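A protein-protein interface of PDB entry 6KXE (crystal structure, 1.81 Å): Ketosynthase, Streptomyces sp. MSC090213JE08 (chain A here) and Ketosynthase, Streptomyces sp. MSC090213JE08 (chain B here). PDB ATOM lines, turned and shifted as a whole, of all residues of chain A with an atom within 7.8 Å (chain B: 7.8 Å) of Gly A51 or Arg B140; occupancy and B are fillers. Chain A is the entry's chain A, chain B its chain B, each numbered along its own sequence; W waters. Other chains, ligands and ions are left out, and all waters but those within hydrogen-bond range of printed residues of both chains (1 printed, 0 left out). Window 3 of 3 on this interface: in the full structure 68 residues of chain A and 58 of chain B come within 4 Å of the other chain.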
ATOM      1  N   THR A  47      18.949 -23.583  -9.623  1.00  0.00           N
ATOM      2  CA  THR A  47      20.136 -23.199 -10.442  1.00  0.00           C
ATOM      3  C   THR A  47      19.781 -22.149 -11.504  1.00  0.00           C
ATOM      4  O   THR A  47      20.705 -21.711 -12.192  1.00  0.00           O
ATOM      5  CB  THR A  47      20.811 -24.425 -11.062  1.00  0.00           C
ATOM      6  OG1 THR A  47      19.826 -25.159 -11.787  1.00  0.00           O
ATOM      7  CG2 THR A  47      21.454 -25.294 -10.011  1.00  0.00           C
ATOM      8  N   GLU A  48      18.512 -21.745 -11.661  1.00  0.00           N
ATOM      9  CA  GLU A  48      18.141 -20.746 -12.710  1.00  0.00           C
ATOM     10  C   GLU A  48      19.019 -19.495 -12.580  1.00  0.00           C
ATOM     11  O   GLU A  48      19.102 -18.953 -11.447  1.00  0.00           O
ATOM     12  CB  GLU A  48      16.679 -20.313 -12.575  1.00  0.00           C
ATOM     13  CG  GLU A  48      16.314 -19.158 -13.500  1.00  0.00           C
ATOM     14  CD  GLU A  48      14.916 -18.592 -13.301  1.00  0.00           C
ATOM     15  OE1 GLU A  48      14.339 -18.799 -12.204  1.00  0.00           O
ATOM     16  OE2 GLU A  48      14.400 -17.945 -14.244  1.00  0.00           O
ATOM     17  N   GLY A  49      19.668 -19.070 -13.671  1.00  0.00           N
ATOM     18  CA  GLY A  49      20.495 -17.848 -13.725  1.00  0.00           C
ATOM     19  C   GLY A  49      21.991 -18.129 -13.607  1.00  0.00           C
ATOM     20  O   GLY A  49      22.762 -17.227 -13.944  1.00  0.00           O
ATOM     21  N   PHE A  50      22.418 -19.333 -13.208  1.00  0.00           N
ATOM     22  CA  PHE A  50      23.868 -19.657 -13.080  1.00  0.00           C
ATOM     23  C   PHE A  50      24.476 -20.002 -14.447  1.00  0.00           C
ATOM     24  O   PHE A  50      25.704 -20.065 -14.542  1.00  0.00           O
ATOM     25  CB  PHE A  50      24.094 -20.789 -12.070  1.00  0.00           C
ATOM     26  CG  PHE A  50      24.015 -20.360 -10.630  1.00  0.00           C
ATOM     27  CD1 PHE A  50      25.094 -19.721 -10.030  1.00  0.00           C
ATOM     28  CD2 PHE A  50      22.878 -20.610  -9.875  1.00  0.00           C
ATOM     29  CE1 PHE A  50      25.012 -19.304  -8.712  1.00  0.00           C
ATOM     30  CE2 PHE A  50      22.816 -20.245  -8.540  1.00  0.00           C
ATOM     31  CZ  PHE A  50      23.890 -19.584  -7.968  1.00  0.00           C
ATOM     32  N   GLY A  51      23.631 -20.346 -15.425  1.00  0.00           N
ATOM     33  CA  GLY A  51      23.991 -20.804 -16.781  1.00  0.00           C
ATOM     34  C   GLY A  51      24.580 -22.201 -16.779  1.00  0.00           C
ATOM     35  O   GLY A  51      25.152 -22.615 -17.771  1.00  0.00           O
ATOM     36  N   GLN A  52      24.565 -22.881 -15.648  1.00  0.00           N
ATOM     37  CA  GLN A  52      25.023 -24.279 -15.552  1.00  0.00           C
ATOM     38  C   GLN A  52      24.344 -24.879 -14.320  1.00  0.00           C
ATOM     39  O   GLN A  52      23.794 -24.120 -13.542  1.00  0.00           O
ATOM     40  CB  GLN A  52      26.551 -24.375 -15.555  1.00  0.00           C
ATOM     41  CG  GLN A  52      27.270 -23.647 -14.429  1.00  0.00           C
ATOM     42  CD  GLN A  52      28.755 -23.496 -14.715  1.00  0.00           C
ATOM     43  OE1 GLN A  52      29.201 -22.450 -15.168  1.00  0.00           O
ATOM     44  NE2 GLN A  52      29.532 -24.543 -14.475  1.00  0.00           N
ATOM     45  N   ASN A  53      24.326 -26.209 -14.191  1.00  0.00           N
ATOM     46  CA  ASN A  53      23.575 -26.842 -13.085  1.00  0.00           C
ATOM     47  C   ASN A  53      24.141 -28.221 -12.738  1.00  0.00           C
ATOM     48  O   ASN A  53      23.327 -29.071 -12.317  1.00  0.00           O
ATOM     49  CB  ASN A  53      22.088 -26.937 -13.432  1.00  0.00           C
ATOM     50  CG  ASN A  53      21.835 -28.018 -14.446  1.00  0.00           C
ATOM     51  OD1 ASN A  53      22.609 -28.166 -15.391  1.00  0.00           O
ATOM     52  ND2 ASN A  53      20.825 -28.835 -14.192  1.00  0.00           N
ATOM     53  N   THR A  54      25.459 -28.411 -12.876  1.00  0.00           N
ATOM     54  CA  THR A  54      26.128 -29.685 -12.547  1.00  0.00           C
ATOM     55  C   THR A  54      26.956 -29.500 -11.265  1.00  0.00           C
ATOM     56  O   THR A  54      27.580 -28.448 -11.119  1.00  0.00           O
ATOM     57  CB  THR A  54      27.023 -30.141 -13.707  1.00  0.00           C
ATOM     58  OG1 THR A  54      26.249 -30.151 -14.906  1.00  0.00           O
ATOM     59  CG2 THR A  54      27.605 -31.513 -13.498  1.00  0.00           C
ATOM     60  N   ARG A 202      24.289 -22.973  -2.458  1.00  0.00           N
ATOM     61  CA  ARG A 202      24.289 -21.795  -3.342  1.00  0.00           C
ATOM     62  C   ARG A 202      25.539 -20.962  -3.083  1.00  0.00           C
ATOM     63  O   ARG A 202      26.163 -20.533  -4.067  1.00  0.00           O
ATOM     64  CB  ARG A 202      23.007 -21.020  -3.059  1.00  0.00           C
ATOM     65  CG  ARG A 202      22.805 -19.763  -3.881  1.00  0.00           C
ATOM     66  CD  ARG A 202      21.419 -19.275  -3.526  1.00  0.00           C
ATOM     67  NE  ARG A 202      21.130 -18.198  -4.418  1.00  0.00           N
ATOM     68  CZ  ARG A 202      20.102 -18.127  -5.224  1.00  0.00           C
ATOM     69  NH1 ARG A 202      19.165 -19.069  -5.279  1.00  0.00           N
ATOM     70  NH2 ARG A 202      19.988 -17.034  -5.928  1.00  0.00           N
ATOM     71  N   PHE A 205      28.612 -22.609  -4.817  1.00  0.00           N
ATOM     72  CA  PHE A 205      28.384 -22.627  -6.283  1.00  0.00           C
ATOM     73  C   PHE A 205      28.551 -21.209  -6.835  1.00  0.00           C
ATOM     74  O   PHE A 205      29.264 -21.042  -7.829  1.00  0.00           O
ATOM     75  CB  PHE A 205      26.985 -23.135  -6.565  1.00  0.00           C
ATOM     76  CG  PHE A 205      26.739 -23.508  -7.997  1.00  0.00           C
ATOM     77  CD1 PHE A 205      27.557 -24.425  -8.625  1.00  0.00           C
ATOM     78  CD2 PHE A 205      25.634 -23.017  -8.672  1.00  0.00           C
ATOM     79  CE1 PHE A 205      27.288 -24.837  -9.921  1.00  0.00           C
ATOM     80  CE2 PHE A 205      25.378 -23.421  -9.974  1.00  0.00           C
ATOM     81  CZ  PHE A 205      26.198 -24.329 -10.589  1.00  0.00           C
ATOM     82  N   ALA A 206      27.935 -20.220  -6.195  1.00  0.00           N
ATOM     83  CA  ALA A 206      27.984 -18.806  -6.638  1.00  0.00           C
ATOM     84  C   ALA A 206      29.427 -18.333  -6.526  1.00  0.00           C
ATOM     85  O   ALA A 206      29.881 -17.618  -7.441  1.00  0.00           O
ATOM     86  CB  ALA A 206      27.056 -17.911  -5.839  1.00  0.00           C
ATOM     87  N   LYS A 209      31.623 -19.888  -9.291  1.00  0.00           N
ATOM     88  CA  LYS A 209      31.155 -19.312 -10.575  1.00  0.00           C
ATOM     89  C   LYS A 209      31.719 -17.892 -10.735  1.00  0.00           C
ATOM     90  O   LYS A 209      32.296 -17.588 -11.807  1.00  0.00           O
ATOM     91  CB  LYS A 209      29.630 -19.316 -10.614  1.00  0.00           C
ATOM     92  CG  LYS A 209      29.039 -18.711 -11.871  1.00  0.00           C
ATOM     93  CD  LYS A 209      29.339 -19.461 -13.114  1.00  0.00           C
ATOM     94  CE  LYS A 209      28.668 -18.741 -14.264  1.00  0.00           C
ATOM     95  NZ  LYS A 209      28.754 -19.531 -15.498  1.00  0.00           N
ATOM     96  N   PRO A 216      32.810 -25.627 -17.331  1.00  0.00           N
ATOM     97  CA  PRO A 216      31.548 -25.635 -18.066  1.00  0.00           C
ATOM     98  C   PRO A 216      31.085 -27.066 -18.356  1.00  0.00           C
ATOM     99  O   PRO A 216      29.956 -27.224 -18.784  1.00  0.00           O
ATOM    100  CB  PRO A 216      31.877 -24.888 -19.379  1.00  0.00           C
ATOM    101  CG  PRO A 216      33.349 -25.196 -19.613  1.00  0.00           C
ATOM    102  CD  PRO A 216      33.961 -25.350 -18.221  1.00  0.00           C
ATOM    103  N   GLN B 134      22.912 -10.597  -2.084  1.00  0.00           N
ATOM    104  CA  GLN B 134      23.226 -10.163  -3.465  1.00  0.00           C
ATOM    105  C   GLN B 134      22.881 -11.292  -4.426  1.00  0.00           C
ATOM    106  O   GLN B 134      22.246 -10.999  -5.467  1.00  0.00           O
ATOM    107  CB  GLN B 134      24.678  -9.741  -3.585  1.00  0.00           C
ATOM    108  CG  GLN B 134      24.950  -8.487  -2.791  1.00  0.00           C
ATOM    109  CD  GLN B 134      26.364  -8.120  -3.096  1.00  0.00           C
ATOM    110  OE1 GLN B 134      27.279  -8.913  -2.860  1.00  0.00           O
ATOM    111  NE2 GLN B 134      26.496  -7.001  -3.803  1.00  0.00           N
ATOM    112  N   SER B 135      23.221 -12.545  -4.089  1.00  0.00           N
ATOM    113  CA  SER B 135      22.833 -13.709  -4.918  1.00  0.00           C
ATOM    114  C   SER B 135      21.322 -13.699  -5.203  1.00  0.00           C
ATOM    115  O   SER B 135      20.941 -14.044  -6.341  1.00  0.00           O
ATOM    116  CB  SER B 135      23.227 -14.987  -4.259  1.00  0.00           C
ATOM    117  OG  SER B 135      22.889 -16.080  -5.076  1.00  0.00           O
ATOM    118  N   TYR B 136      20.481 -13.450  -4.186  1.00  0.00           N
ATOM    119  CA  TYR B 136      19.007 -13.578  -4.269  1.00  0.00           C
ATOM    120  C   TYR B 136      18.417 -12.393  -5.041  1.00  0.00           C
ATOM    121  O   TYR B 136      17.417 -12.628  -5.746  1.00  0.00           O
ATOM    122  CB  TYR B 136      18.361 -13.755  -2.888  1.00  0.00           C
ATOM    123  CG  TYR B 136      18.423 -15.180  -2.399  1.00  0.00           C
ATOM    124  CD1 TYR B 136      17.702 -16.188  -3.024  1.00  0.00           C
ATOM    125  CD2 TYR B 136      19.248 -15.549  -1.345  1.00  0.00           C
ATOM    126  CE1 TYR B 136      17.784 -17.511  -2.604  1.00  0.00           C
ATOM    127  CE2 TYR B 136      19.330 -16.869  -0.907  1.00  0.00           C
ATOM    128  CZ  TYR B 136      18.602 -17.860  -1.544  1.00  0.00           C
ATOM    129  OH  TYR B 136      18.659 -19.163  -1.099  1.00  0.00           O
ATOM    130  N   THR B 137      19.019 -11.213  -4.954  1.00  0.00           N
ATOM    131  CA  THR B 137      18.393  -9.915  -5.345  1.00  0.00           C
ATOM    132  C   THR B 137      19.042  -9.271  -6.591  1.00  0.00           C
ATOM    133  O   THR B 137      18.422  -8.372  -7.132  1.00  0.00           O
ATOM    134  CB  THR B 137      18.353  -8.925  -4.165  1.00  0.00           C
ATOM    135  OG1 THR B 137      19.643  -8.456  -3.806  1.00  0.00           O
ATOM    136  CG2 THR B 137      17.723  -9.518  -2.928  1.00  0.00           C
ATOM    137  N   ASN B 138      20.235  -9.675  -7.046  1.00  0.00           N
ATOM    138  CA  ASN B 138      20.874  -9.028  -8.218  1.00  0.00           C
ATOM    139  C   ASN B 138      20.364  -9.748  -9.470  1.00  0.00           C
ATOM    140  O   ASN B 138      19.543 -10.677  -9.341  1.00  0.00           O
ATOM    141  CB  ASN B 138      22.391  -8.911  -8.026  1.00  0.00           C
ATOM    142  CG  ASN B 138      22.724  -7.827  -7.021  1.00  0.00           C
ATOM    143  OD1 ASN B 138      21.885  -6.969  -6.752  1.00  0.00           O
ATOM    144  ND2 ASN B 138      23.932  -7.821  -6.479  1.00  0.00           N
ATOM    145  N   ALA B 139      20.782  -9.298 -10.640  1.00  0.00           N
ATOM    146  CA  ALA B 139      20.196  -9.750 -11.927  1.00  0.00           C
ATOM    147  C   ALA B 139      20.463 -11.244 -12.152  1.00  0.00           C
ATOM    148  O   ALA B 139      19.620 -11.947 -12.793  1.00  0.00           O
ATOM    149  CB  ALA B 139      20.723  -8.874 -13.048  1.00  0.00           C
ATOM    150  N   ARG B 140      21.601 -11.744 -11.679  1.00  0.00           N
ATOM    151  CA  ARG B 140      21.923 -13.181 -11.753  1.00  0.00           C
ATOM    152  C   ARG B 140      22.509 -13.599 -10.406  1.00  0.00           C
ATOM    153  O   ARG B 140      23.032 -12.753  -9.683  1.00  0.00           O
ATOM    154  CB  ARG B 140      22.851 -13.426 -12.939  1.00  0.00           C
ATOM    155  CG  ARG B 140      22.123 -13.284 -14.273  1.00  0.00           C
ATOM    156  CD  ARG B 140      23.017 -13.501 -15.439  1.00  0.00           C
ATOM    157  NE  ARG B 140      23.356 -14.898 -15.595  1.00  0.00           N
ATOM    158  CZ  ARG B 140      24.433 -15.351 -16.226  1.00  0.00           C
ATOM    159  NH1 ARG B 140      25.344 -14.509 -16.694  1.00  0.00           N
ATOM    160  NH2 ARG B 140      24.618 -16.657 -16.363  1.00  0.00           N
ATOM    161  N   PRO B 141      22.376 -14.887 -10.035  1.00  0.00           N
ATOM    162  CA  PRO B 141      22.642 -15.328  -8.664  1.00  0.00           C
ATOM    163  C   PRO B 141      24.121 -15.492  -8.267  1.00  0.00           C
ATOM    164  O   PRO B 141      24.409 -15.838  -7.102  1.00  0.00           O
ATOM    165  CB  PRO B 141      21.863 -16.655  -8.571  1.00  0.00           C
ATOM    166  CG  PRO B 141      21.796 -17.165  -9.989  1.00  0.00           C
ATOM    167  CD  PRO B 141      21.764 -15.940 -10.865  1.00  0.00           C
ATOM    168  N   PHE B 142      25.053 -15.177  -9.163  1.00  0.00           N
ATOM    169  CA  PHE B 142      26.486 -15.025  -8.807  1.00  0.00           C
ATOM    170  C   PHE B 142      26.966 -13.587  -9.005  1.00  0.00           C
ATOM    171  O   PHE B 142      28.194 -13.385  -9.014  1.00  0.00           O
ATOM    172  CB  PHE B 142      27.310 -16.011  -9.624  1.00  0.00           C
ATOM    173  CG  PHE B 142      27.254 -15.821 -11.114  1.00  0.00           C
ATOM    174  CD1 PHE B 142      26.207 -16.365 -11.866  1.00  0.00           C
ATOM    175  CD2 PHE B 142      28.283 -15.185 -11.772  1.00  0.00           C
ATOM    176  CE1 PHE B 142      26.181 -16.220 -13.245  1.00  0.00           C
ATOM    177  CE2 PHE B 142      28.265 -15.068 -13.156  1.00  0.00           C
ATOM    178  CZ  PHE B 142      27.208 -15.561 -13.876  1.00  0.00           C
ATOM    179  N   TYR B 143      26.048 -12.633  -9.175  1.00  0.00           N
ATOM    180  CA  TYR B 143      26.355 -11.193  -9.368  1.00  0.00           C
ATOM    181  C   TYR B 143      26.468 -10.569  -7.989  1.00  0.00           C
ATOM    182  O   TYR B 143      25.583  -9.849  -7.520  1.00  0.00           O
ATOM    183  CB  TYR B 143      25.337 -10.462 -10.242  1.00  0.00           C
ATOM    184  CG  TYR B 143      25.475 -10.745 -11.714  1.00  0.00           C
ATOM    185  CD1 TYR B 143      26.301 -11.756 -12.198  1.00  0.00           C
ATOM    186  CD2 TYR B 143      24.708 -10.073 -12.641  1.00  0.00           C
ATOM    187  CE1 TYR B 143      26.450 -11.996 -13.549  1.00  0.00           C
ATOM    188  CE2 TYR B 143      24.795 -10.352 -14.004  1.00  0.00           C
ATOM    189  CZ  TYR B 143      25.671 -11.313 -14.466  1.00  0.00           C
ATOM    190  OH  TYR B 143      25.797 -11.583 -15.807  1.00  0.00           O
ATOM    191  N   VAL B 144      27.610 -10.832  -7.373  1.00  0.00           N
ATOM    192  CA  VAL B 144      27.902 -10.409  -5.972  1.00  0.00           C
ATOM    193  C   VAL B 144      29.072  -9.433  -5.969  1.00  0.00           C
ATOM    194  O   VAL B 144      29.693  -9.219  -7.004  1.00  0.00           O
ATOM    195  CB  VAL B 144      28.178 -11.627  -5.079  1.00  0.00           C
ATOM    196  CG1 VAL B 144      27.014 -12.594  -5.091  1.00  0.00           C
ATOM    197  CG2 VAL B 144      29.442 -12.352  -5.483  1.00  0.00           C
HETATM  198  O   HOH W   1      22.098 -17.970 -17.197  1.00  0.00           O
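Of the printed residues of chain B, Glu A48 touches Pro B141.
Of the printed residues of chain B, Phe A50 touches Arg B140 (3.9 Å), Pro B141 (3.6 Å) and Phe B142 (3.98 Å).
Of chain B, only Arg B140 comes within 4 Å of Gly A51.
Of the printed residues of chain B, Ala A206 touches Pro B141 and Phe B142.
Printed residues of chain A within 4 Å of Ser B135: Arg A202 (2.8 Å).
No residue of chain A comes within 4 Å of Ala B139.
Of the printed residues of chain A, Arg B140 touches Gly A49, Phe A50 and Gly A51.
O of Gly A49 sits at hydrogen-bond distance from NE of Arg B140, 2.9 Å away.
The side-chain hydroxyl (OG) of Ser B135 sits at hydrogen-bond distance from the guanidinium group (NE) of Arg A202 (2.8 Å).
Among the printed residues, pairs that only touch across the chains: Glu A48 with Pro B141, Gly A49 with Pro B141, Gly A49 with Phe B142, Phe A50 with Arg B140, Phe A50 with Pro B141, Phe A50 with Phe B142, Gly A51 with Arg B140, Arg A202 with Tyr B136, Arg A202 with Pro B141, Ala A206 with Pro B141, Ala A206 with Phe B142 and Lys A209 with Phe B142.
NZ of Lys A209 is in hydrogen-bond range of O of Phe A50, at 3.2 Å.
The side-chain amide oxygen (OE1) of Gln A52 is in hydrogen-bond range of the side-chain amino group (NZ) of Lys A209, 3.0 Å away.
The backbone carbonyl oxygen (O) of Pro B141 sits at hydrogen-bond distance from the side-chain hydroxyl (OG) of Ser B135 (2.5 Å).
The side-chain hydroxyl of Tyr B143 lies within hydrogen-bond range of the guanidinium group of Arg B140 (3.1 Å).
Water W1 lies within hydrogen-bond range of NH2 of Arg B140 (3.0 Å), N of Gly A51 (3.3 Å) and O of Gly A49 (3.4 Å).
Hydrophobic or aromatic side chains of chain A within 4 Å of the printed part of chain B: Phe A50 and Ala A206.
Hydrophobic or aromatic side chains of chain B that line the printed part of chain A: Tyr B136, Pro B141 and Phe B142.
Among the printed residues, 14 pairs touch across the chains.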
